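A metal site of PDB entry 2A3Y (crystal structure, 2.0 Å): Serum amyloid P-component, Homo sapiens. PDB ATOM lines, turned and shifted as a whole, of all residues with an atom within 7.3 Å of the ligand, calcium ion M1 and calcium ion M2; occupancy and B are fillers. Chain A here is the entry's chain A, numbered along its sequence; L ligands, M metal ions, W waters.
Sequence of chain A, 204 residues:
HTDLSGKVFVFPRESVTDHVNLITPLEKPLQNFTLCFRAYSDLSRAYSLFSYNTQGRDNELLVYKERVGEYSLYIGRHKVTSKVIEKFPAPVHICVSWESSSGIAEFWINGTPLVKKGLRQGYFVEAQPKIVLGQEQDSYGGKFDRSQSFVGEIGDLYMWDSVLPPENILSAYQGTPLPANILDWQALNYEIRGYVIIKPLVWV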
ATOM      1  N   SER A  48     -23.957  -0.289   0.523  1.00  0.00           N
ATOM      2  CA  SER A  48     -23.421   0.722   1.435  1.00  0.00           C
ATOM      3  C   SER A  48     -23.933   2.111   1.063  1.00  0.00           C
ATOM      4  O   SER A  48     -23.920   2.494  -0.109  1.00  0.00           O
ATOM      5  CB  SER A  48     -21.893   0.712   1.392  1.00  0.00           C
ATOM      6  OG  SER A  48     -21.340   1.679   2.269  1.00  0.00           O
ATOM      7  N   SER A  51     -19.688   4.963   3.938  1.00  0.00           N
ATOM      8  CA  SER A  51     -18.580   4.132   4.412  1.00  0.00           C
ATOM      9  C   SER A  51     -17.435   5.004   4.937  1.00  0.00           C
ATOM     10  O   SER A  51     -16.881   5.831   4.214  1.00  0.00           O
ATOM     11  CB  SER A  51     -18.103   3.185   3.315  1.00  0.00           C
ATOM     12  OG  SER A  51     -16.897   2.528   3.674  1.00  0.00           O
ATOM     13  N   ASN A  53     -13.958   4.555   7.042  1.00  0.00           N
ATOM     14  CA  ASN A  53     -12.907   3.676   7.548  1.00  0.00           C
ATOM     15  C   ASN A  53     -11.726   4.491   8.037  1.00  0.00           C
ATOM     16  O   ASN A  53     -11.466   5.590   7.528  1.00  0.00           O
ATOM     17  CB  ASN A  53     -12.433   2.717   6.439  1.00  0.00           C
ATOM     18  CG  ASN A  53     -13.256   1.441   6.361  1.00  0.00           C
ATOM     19  OD1 ASN A  53     -14.395   1.382   6.814  1.00  0.00           O
ATOM     20  ND2 ASN A  53     -12.666   0.406   5.751  1.00  0.00           N
ATOM     21  N   ASP A  58     -11.514  -1.425   9.582  1.00  0.00           N
ATOM     22  CA  ASP A  58     -12.653  -1.569   8.684  1.00  0.00           C
ATOM     23  C   ASP A  58     -13.953  -1.324   9.441  1.00  0.00           C
ATOM     24  O   ASP A  58     -14.034  -1.574  10.647  1.00  0.00           O
ATOM     25  CB  ASP A  58     -12.651  -2.970   8.067  1.00  0.00           C
ATOM     26  CG  ASP A  58     -13.764  -3.156   7.043  1.00  0.00           C
ATOM     27  OD1 ASP A  58     -13.933  -2.273   6.188  1.00  0.00           O
ATOM     28  OD2 ASP A  58     -14.508  -4.159   7.032  1.00  0.00           O
ATOM     29  N   ASN A  59     -14.976  -0.839   8.736  1.00  0.00           N
ATOM     30  CA  ASN A  59     -16.307  -0.603   9.298  1.00  0.00           C
ATOM     31  C   ASN A  59     -16.283   0.196  10.608  1.00  0.00           C
ATOM     32  O   ASN A  59     -16.971  -0.140  11.569  1.00  0.00           O
ATOM     33  CB  ASN A  59     -17.059  -1.934   9.488  1.00  0.00           C
ATOM     34  CG  ASN A  59     -17.210  -2.717   8.196  1.00  0.00           C
ATOM     35  OD1 ASN A  59     -16.870  -2.234   7.109  1.00  0.00           O
ATOM     36  ND2 ASN A  59     -17.726  -3.935   8.297  1.00  0.00           N
ATOM     37  N   GLU A  60     -15.457   1.235  10.627  1.00  0.00           N
ATOM     38  CA  GLU A  60     -15.377   2.130  11.780  1.00  0.00           C
ATOM     39  C   GLU A  60     -16.703   2.872  11.962  1.00  0.00           C
ATOM     40  O   GLU A  60     -17.213   2.984  13.075  1.00  0.00           O
ATOM     41  CB  GLU A  60     -14.227   3.119  11.634  1.00  0.00           C
ATOM     42  CG  GLU A  60     -13.891   3.909  12.894  1.00  0.00           C
ATOM     43  CD  GLU A  60     -13.472   3.034  14.072  1.00  0.00           C
ATOM     44  OE1 GLU A  60     -13.120   1.853  13.869  1.00  0.00           O
ATOM     45  OE2 GLU A  60     -13.495   3.544  15.213  1.00  0.00           O
ATOM     46  N   LEU A  62     -20.262   2.844   9.503  1.00  0.00           N
ATOM     47  CA  LEU A  62     -20.864   2.373   8.262  1.00  0.00           C
ATOM     48  C   LEU A  62     -22.379   2.375   8.345  1.00  0.00           C
ATOM     49  O   LEU A  62     -22.958   1.815   9.272  1.00  0.00           O
ATOM     50  CB  LEU A  62     -20.327   0.978   7.918  1.00  0.00           C
ATOM     51  CG  LEU A  62     -20.978   0.165   6.794  1.00  0.00           C
ATOM     52  CD1 LEU A  62     -20.730   0.820   5.433  1.00  0.00           C
ATOM     53  CD2 LEU A  62     -20.451  -1.260   6.800  1.00  0.00           C
ATOM     54  N   TYR A  64     -25.434   0.900   6.321  1.00  0.00           N
ATOM     55  CA  TYR A  64     -25.569  -0.226   5.410  1.00  0.00           C
ATOM     56  C   TYR A  64     -27.017  -0.690   5.307  1.00  0.00           C
ATOM     57  O   TYR A  64     -27.660  -0.993   6.314  1.00  0.00           O
ATOM     58  CB  TYR A  64     -24.687  -1.379   5.927  1.00  0.00           C
ATOM     59  CG  TYR A  64     -24.424  -2.498   4.941  1.00  0.00           C
ATOM     60  CD1 TYR A  64     -23.511  -2.334   3.887  1.00  0.00           C
ATOM     61  CD2 TYR A  64     -25.049  -3.737   5.077  1.00  0.00           C
ATOM     62  CE1 TYR A  64     -23.257  -3.374   2.992  1.00  0.00           C
ATOM     63  CE2 TYR A  64     -24.795  -4.777   4.181  1.00  0.00           C
ATOM     64  CZ  TYR A  64     -23.898  -4.590   3.150  1.00  0.00           C
ATOM     65  OH  TYR A  64     -23.646  -5.609   2.267  1.00  0.00           O
ATOM     66  N   GLU A  66     -29.368  -3.506   4.405  1.00  0.00           N
ATOM     67  CA  GLU A  66     -29.384  -4.966   4.264  1.00  0.00           C
ATOM     68  C   GLU A  66     -30.324  -5.439   3.161  1.00  0.00           C
ATOM     69  O   GLU A  66     -29.978  -6.268   2.326  1.00  0.00           O
ATOM     70  CB  GLU A  66     -29.819  -5.610   5.580  1.00  0.00           C
ATOM     71  CG  GLU A  66     -29.039  -5.186   6.811  1.00  0.00           C
ATOM     72  CD  GLU A  66     -27.661  -5.805   6.878  1.00  0.00           C
ATOM     73  OE1 GLU A  66     -27.431  -6.850   6.234  1.00  0.00           O
ATOM     74  OE2 GLU A  66     -26.802  -5.236   7.587  1.00  0.00           O
ATOM     75  N   TYR A  74     -22.995   0.354  11.661  1.00  0.00           N
ATOM     76  CA  TYR A  74     -21.794  -0.234  12.229  1.00  0.00           C
ATOM     77  C   TYR A  74     -21.017   0.854  12.968  1.00  0.00           C
ATOM     78  O   TYR A  74     -20.794   1.924  12.414  1.00  0.00           O
ATOM     79  CB  TYR A  74     -20.911  -0.840  11.139  1.00  0.00           C
ATOM     80  CG  TYR A  74     -21.436  -2.132  10.536  1.00  0.00           C
ATOM     81  CD1 TYR A  74     -22.513  -2.126   9.659  1.00  0.00           C
ATOM     82  CD2 TYR A  74     -20.841  -3.350  10.842  1.00  0.00           C
ATOM     83  CE1 TYR A  74     -22.993  -3.304   9.101  1.00  0.00           C
ATOM     84  CE2 TYR A  74     -21.311  -4.546  10.293  1.00  0.00           C
ATOM     85  CZ  TYR A  74     -22.394  -4.509   9.419  1.00  0.00           C
ATOM     86  OH  TYR A  74     -22.863  -5.669   8.874  1.00  0.00           O
ATOM     87  N   ARG A  77     -16.938  -1.861  13.939  1.00  0.00           N
ATOM     88  CA  ARG A  77     -17.186  -3.259  13.575  1.00  0.00           C
ATOM     89  C   ARG A  77     -18.424  -3.907  14.213  1.00  0.00           C
ATOM     90  O   ARG A  77     -18.916  -4.911  13.707  1.00  0.00           O
ATOM     91  CB  ARG A  77     -15.933  -4.129  13.777  1.00  0.00           C
ATOM     92  CG  ARG A  77     -14.861  -3.862  12.732  1.00  0.00           C
ATOM     93  CD  ARG A  77     -13.421  -3.804  13.238  1.00  0.00           C
ATOM     94  NE  ARG A  77     -13.212  -2.915  14.395  1.00  0.00           N
ATOM     95  CZ  ARG A  77     -13.143  -1.591  14.339  1.00  0.00           C
ATOM     96  NH1 ARG A  77     -13.290  -0.933  13.195  1.00  0.00           N
ATOM     97  NH2 ARG A  77     -12.934  -0.896  15.462  1.00  0.00           N
ATOM     98  N   LYS A  79     -22.450  -4.003  15.116  1.00  0.00           N
ATOM     99  CA  LYS A  79     -23.573  -3.676  14.246  1.00  0.00           C
ATOM    100  C   LYS A  79     -24.908  -3.671  14.992  1.00  0.00           C
ATOM    101  O   LYS A  79     -25.145  -4.514  15.867  1.00  0.00           O
ATOM    102  CB  LYS A  79     -23.587  -4.656  13.056  1.00  0.00           C
ATOM    103  CG  LYS A  79     -24.899  -4.812  12.310  1.00  0.00           C
ATOM    104  CD  LYS A  79     -24.950  -6.168  11.626  1.00  0.00           C
ATOM    105  CE  LYS A  79     -25.996  -6.216  10.542  1.00  0.00           C
ATOM    106  NZ  LYS A  79     -25.546  -7.020   9.370  1.00  0.00           N
ATOM    107  N   GLU A 136     -18.485   0.305  -0.645  1.00  0.00           N
ATOM    108  CA  GLU A 136     -18.133  -0.102   0.699  1.00  0.00           C
ATOM    109  C   GLU A 136     -16.623  -0.368   0.785  1.00  0.00           C
ATOM    110  O   GLU A 136     -16.080  -1.170   0.021  1.00  0.00           O
ATOM    111  CB  GLU A 136     -18.908  -1.352   1.110  1.00  0.00           C
ATOM    112  CG  GLU A 136     -19.240  -1.441   2.599  1.00  0.00           C
ATOM    113  CD  GLU A 136     -18.090  -1.970   3.434  1.00  0.00           C
ATOM    114  OE1 GLU A 136     -17.435  -2.950   3.006  1.00  0.00           O
ATOM    115  OE2 GLU A 136     -17.845  -1.413   4.521  1.00  0.00           O
ATOM    116  N   GLN A 137     -15.957   0.311   1.721  1.00  0.00           N
ATOM    117  CA  GLN A 137     -14.524   0.117   1.913  1.00  0.00           C
ATOM    118  C   GLN A 137     -14.247  -1.131   2.748  1.00  0.00           C
ATOM    119  O   GLN A 137     -14.973  -1.419   3.693  1.00  0.00           O
ATOM    120  CB  GLN A 137     -13.918   1.302   2.658  1.00  0.00           C
ATOM    121  CG  GLN A 137     -13.833   2.593   1.883  1.00  0.00           C
ATOM    122  CD  GLN A 137     -13.470   3.747   2.796  1.00  0.00           C
ATOM    123  OE1 GLN A 137     -12.299   4.025   3.017  1.00  0.00           O
ATOM    124  NE2 GLN A 137     -14.485   4.400   3.352  1.00  0.00           N
ATOM    125  N   ASP A 138     -13.188  -1.861   2.396  1.00  0.00           N
ATOM    126  CA  ASP A 138     -12.643  -2.897   3.266  1.00  0.00           C
ATOM    127  C   ASP A 138     -11.216  -2.560   3.696  1.00  0.00           C
ATOM    128  O   ASP A 138     -10.661  -3.177   4.609  1.00  0.00           O
ATOM    129  CB  ASP A 138     -12.722  -4.273   2.619  1.00  0.00           C
ATOM    130  CG  ASP A 138     -14.131  -4.837   2.586  1.00  0.00           C
ATOM    131  OD1 ASP A 138     -14.978  -4.428   3.421  1.00  0.00           O
ATOM    132  OD2 ASP A 138     -14.496  -5.699   1.760  1.00  0.00           O
ATOM    133  N   SER A 139     -10.628  -1.579   3.023  1.00  0.00           N
ATOM    134  CA  SER A 139      -9.316  -1.047   3.381  1.00  0.00           C
ATOM    135  C   SER A 139      -9.429   0.455   3.633  1.00  0.00           C
ATOM    136  O   SER A 139     -10.520   1.025   3.530  1.00  0.00           O
ATOM    137  CB  SER A 139      -8.303  -1.331   2.275  1.00  0.00           C
ATOM    138  OG  SER A 139      -8.456  -0.417   1.203  1.00  0.00           O
ATOM    139  N   GLY A 142     -10.156   1.935   0.087  1.00  0.00           N
ATOM    140  CA  GLY A 142     -10.358   1.023  -1.021  1.00  0.00           C
ATOM    141  C   GLY A 142     -10.862  -0.365  -0.678  1.00  0.00           C
ATOM    142  O   GLY A 142     -11.631  -0.539   0.280  1.00  0.00           O
ATOM    143  N   LYS A 143     -10.397  -1.352  -1.448  1.00  0.00           N
ATOM    144  CA  LYS A 143     -10.884  -2.735  -1.395  1.00  0.00           C
ATOM    145  C   LYS A 143     -12.403  -2.777  -1.469  1.00  0.00           C
ATOM    146  O   LYS A 143     -13.089  -3.271  -0.548  1.00  0.00           O
ATOM    147  CB  LYS A 143     -10.322  -3.483  -0.176  1.00  0.00           C
ATOM    148  CG  LYS A 143      -8.877  -3.970  -0.352  1.00  0.00           C
ATOM    149  CD  LYS A 143      -8.480  -4.954   0.752  1.00  0.00           C
ATOM    150  CE  LYS A 143      -6.966  -5.038   0.900  1.00  0.00           C
ATOM    151  NZ  LYS A 143      -6.565  -6.118   1.831  1.00  0.00           N
ATOM    152  N   PHE A 144     -12.927  -2.240  -2.562  1.00  0.00           N
ATOM    153  CA  PHE A 144     -14.368  -2.130  -2.775  1.00  0.00           C
ATOM    154  C   PHE A 144     -14.965  -3.469  -3.216  1.00  0.00           C
ATOM    155  O   PHE A 144     -14.231  -4.400  -3.565  1.00  0.00           O
ATOM    156  CB  PHE A 144     -14.662  -1.034  -3.820  1.00  0.00           C
ATOM    157  CG  PHE A 144     -14.153   0.329  -3.441  1.00  0.00           C
ATOM    158  CD1 PHE A 144     -14.327   0.829  -2.145  1.00  0.00           C
ATOM    159  CD2 PHE A 144     -13.516   1.133  -4.376  1.00  0.00           C
ATOM    160  CE1 PHE A 144     -13.860   2.090  -1.800  1.00  0.00           C
ATOM    161  CE2 PHE A 144     -13.049   2.395  -4.040  1.00  0.00           C
ATOM    162  CZ  PHE A 144     -13.226   2.882  -2.747  1.00  0.00           C
ATOM    163  N   ASP A 145     -16.289  -3.548  -3.186  1.00  0.00           N
ATOM    164  CA  ASP A 145     -17.004  -4.782  -3.517  1.00  0.00           C
ATOM    165  C   ASP A 145     -18.213  -4.446  -4.389  1.00  0.00           C
ATOM    166  O   ASP A 145     -19.134  -3.749  -3.955  1.00  0.00           O
ATOM    167  CB  ASP A 145     -17.429  -5.497  -2.230  1.00  0.00           C
ATOM    168  CG  ASP A 145     -18.111  -6.846  -2.484  1.00  0.00           C
ATOM    169  OD1 ASP A 145     -18.553  -7.129  -3.625  1.00  0.00           O
ATOM    170  OD2 ASP A 145     -18.274  -7.685  -1.575  1.00  0.00           O
ATOM    171  N   GLN A 148     -21.750  -4.702  -3.205  1.00  0.00           N
ATOM    172  CA  GLN A 148     -22.086  -3.776  -2.125  1.00  0.00           C
ATOM    173  C   GLN A 148     -22.171  -2.323  -2.614  1.00  0.00           C
ATOM    174  O   GLN A 148     -22.474  -1.416  -1.838  1.00  0.00           O
ATOM    175  CB  GLN A 148     -21.082  -3.887  -0.981  1.00  0.00           C
ATOM    176  CG  GLN A 148     -21.167  -5.202  -0.189  1.00  0.00           C
ATOM    177  CD  GLN A 148     -20.063  -5.347   0.844  1.00  0.00           C
ATOM    178  OE1 GLN A 148     -18.936  -4.890   0.641  1.00  0.00           O
ATOM    179  NE2 GLN A 148     -20.379  -6.016   1.949  1.00  0.00           N
HETATM  180  C1  LIG L   1     -20.595 -11.225   6.671  1.00  0.00           C
HETATM  181  O1  LIG L   1     -20.221 -12.348   6.375  1.00  0.00           O
HETATM  182  O2  LIG L   1     -19.673 -10.104   6.552  1.00  0.00           O
HETATM  183  C2  LIG L   1     -20.175  -8.779   6.415  1.00  0.00           C
HETATM  184  C3  LIG L   1     -19.307  -7.816   7.192  1.00  0.00           C
HETATM  185  O3  LIG L   1     -19.743  -6.469   6.989  1.00  0.00           O
HETATM  186  C4  LIG L   1     -20.123  -8.367   4.945  1.00  0.00           C
HETATM  187  O4  LIG L   1     -20.541  -7.005   4.805  1.00  0.00           O
HETATM  188  C5  LIG L   1     -19.868  -6.031   5.617  1.00  0.00           C
HETATM  189  C6  LIG L   1     -20.726  -4.777   5.618  1.00  0.00           C
HETATM  190  C7  LIG L   1     -18.512  -5.680   5.036  1.00  0.00           C
HETATM  191  O5  LIG L   1     -18.318  -5.827   3.816  1.00  0.00           O
HETATM  192  O6  LIG L   1     -17.627  -5.230   5.812  1.00  0.00           O
HETATM  193 CA    CA M   1     -15.930  -3.055   5.037  1.00  0.00          CA
HETATM  194 CA    CA M   2     -16.823  -4.955   1.884  1.00  0.00          CA
HETATM  195  O   HOH W   1     -17.062  -7.129   0.849  1.00  0.00           O
HETATM  196  O   HOH W   2     -15.937  -3.779   0.208  1.00  0.00           O
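NE2 of Gln 148 is in hydrogen-bond range of OH of Tyr 64, 3.3 Å away.
The backbone carbonyl oxygen (O) of Gln 148 lies within hydrogen-bond range of the backbone NH (N) of Ser 48.
ND2 of Asn 53 sits close to OD1 of Asp 58 (3.0 Å).
N of Arg 77 is in hydrogen-bond range of O of Asn 59 (2.9 Å).
The side-chain hydroxyl (OH) of Tyr 74 is in hydrogen-bond range of the side-chain amino group (NZ) of Lys 79 (3.0 Å).
NE2 of Gln 137 sits at hydrogen-bond distance from O of Ser 51.
The backbone carbonyl oxygen of Leu 62 is in hydrogen-bond range of the backbone NH of Tyr 74, at 2.8 Å.
The guanidinium group (NH1) of Arg 77 sits at hydrogen-bond distance from the backbone carbonyl oxygen (O) of Asp 58, 2.7 Å away.
Leu 62 touches the ligand.
Tyr 64 touches the ligand (CE1 to C6, 3.9 Å).
Tyr 74 touches the ligand.
Hydrophobic or aromatic side chains within 4 Å of the ligand: Leu 62 and Tyr 64.
Within 4 Å of the ligand: Asp 58, Asn 59, Leu 62, Tyr 64, Tyr 74, Glu 136, Asp 138 and Gln 148.
Within 4 Å of calcium ion M1: Asp 58, Asn 59, Glu 136, Gln 137 and Asp 138.
Along chain A the residues within 4 Å of calcium ion M1 span positions 58 to 138.
Three residues have an atom within 4 Å of calcium ion M2: Glu 136, Asp 138 and Gln 148.
Calcium ion M1 is bound by the side-chain carboxylate (OD1) of Asp 138, the backbone carbonyl oxygen (O) of Gln 137, the side-chain amide oxygen (OD1) of Asn 59, the side-chain carboxylate (OD1) of Asp 58, the side-chain carboxylate (OE1) of Glu 136, the side-chain carboxylate (OE2) of Glu 136, the side-chain carboxylate (OD2) of Asp 58 and an oxygen (O6) of the ligand.
Calcium ion M1 has eight donor atoms within binding distance.
Calcium ion M2 is bound by water W2 (2.2 Å), the side-chain carboxylate (OE1) of Glu 136 (2.4 Å), water W1 (2.4 Å), the side-chain carboxylate (OD2) of Asp 138 (2.4 Å), the side-chain amide oxygen (OE1) of Gln 148 (2.5 Å), the side-chain carboxylate (OD1) of Asp 138 (2.5 Å) and an oxygen (O5) of the ligand (2.6 Å).
Water W2 lies within hydrogen-bond range of the backbone carbonyl oxygen of Glu 136 (2.6 Å), the backbone carbonyl oxygen of Lys 143 (3.0 Å) and the backbone NH of Asp 145 (3.4 Å).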
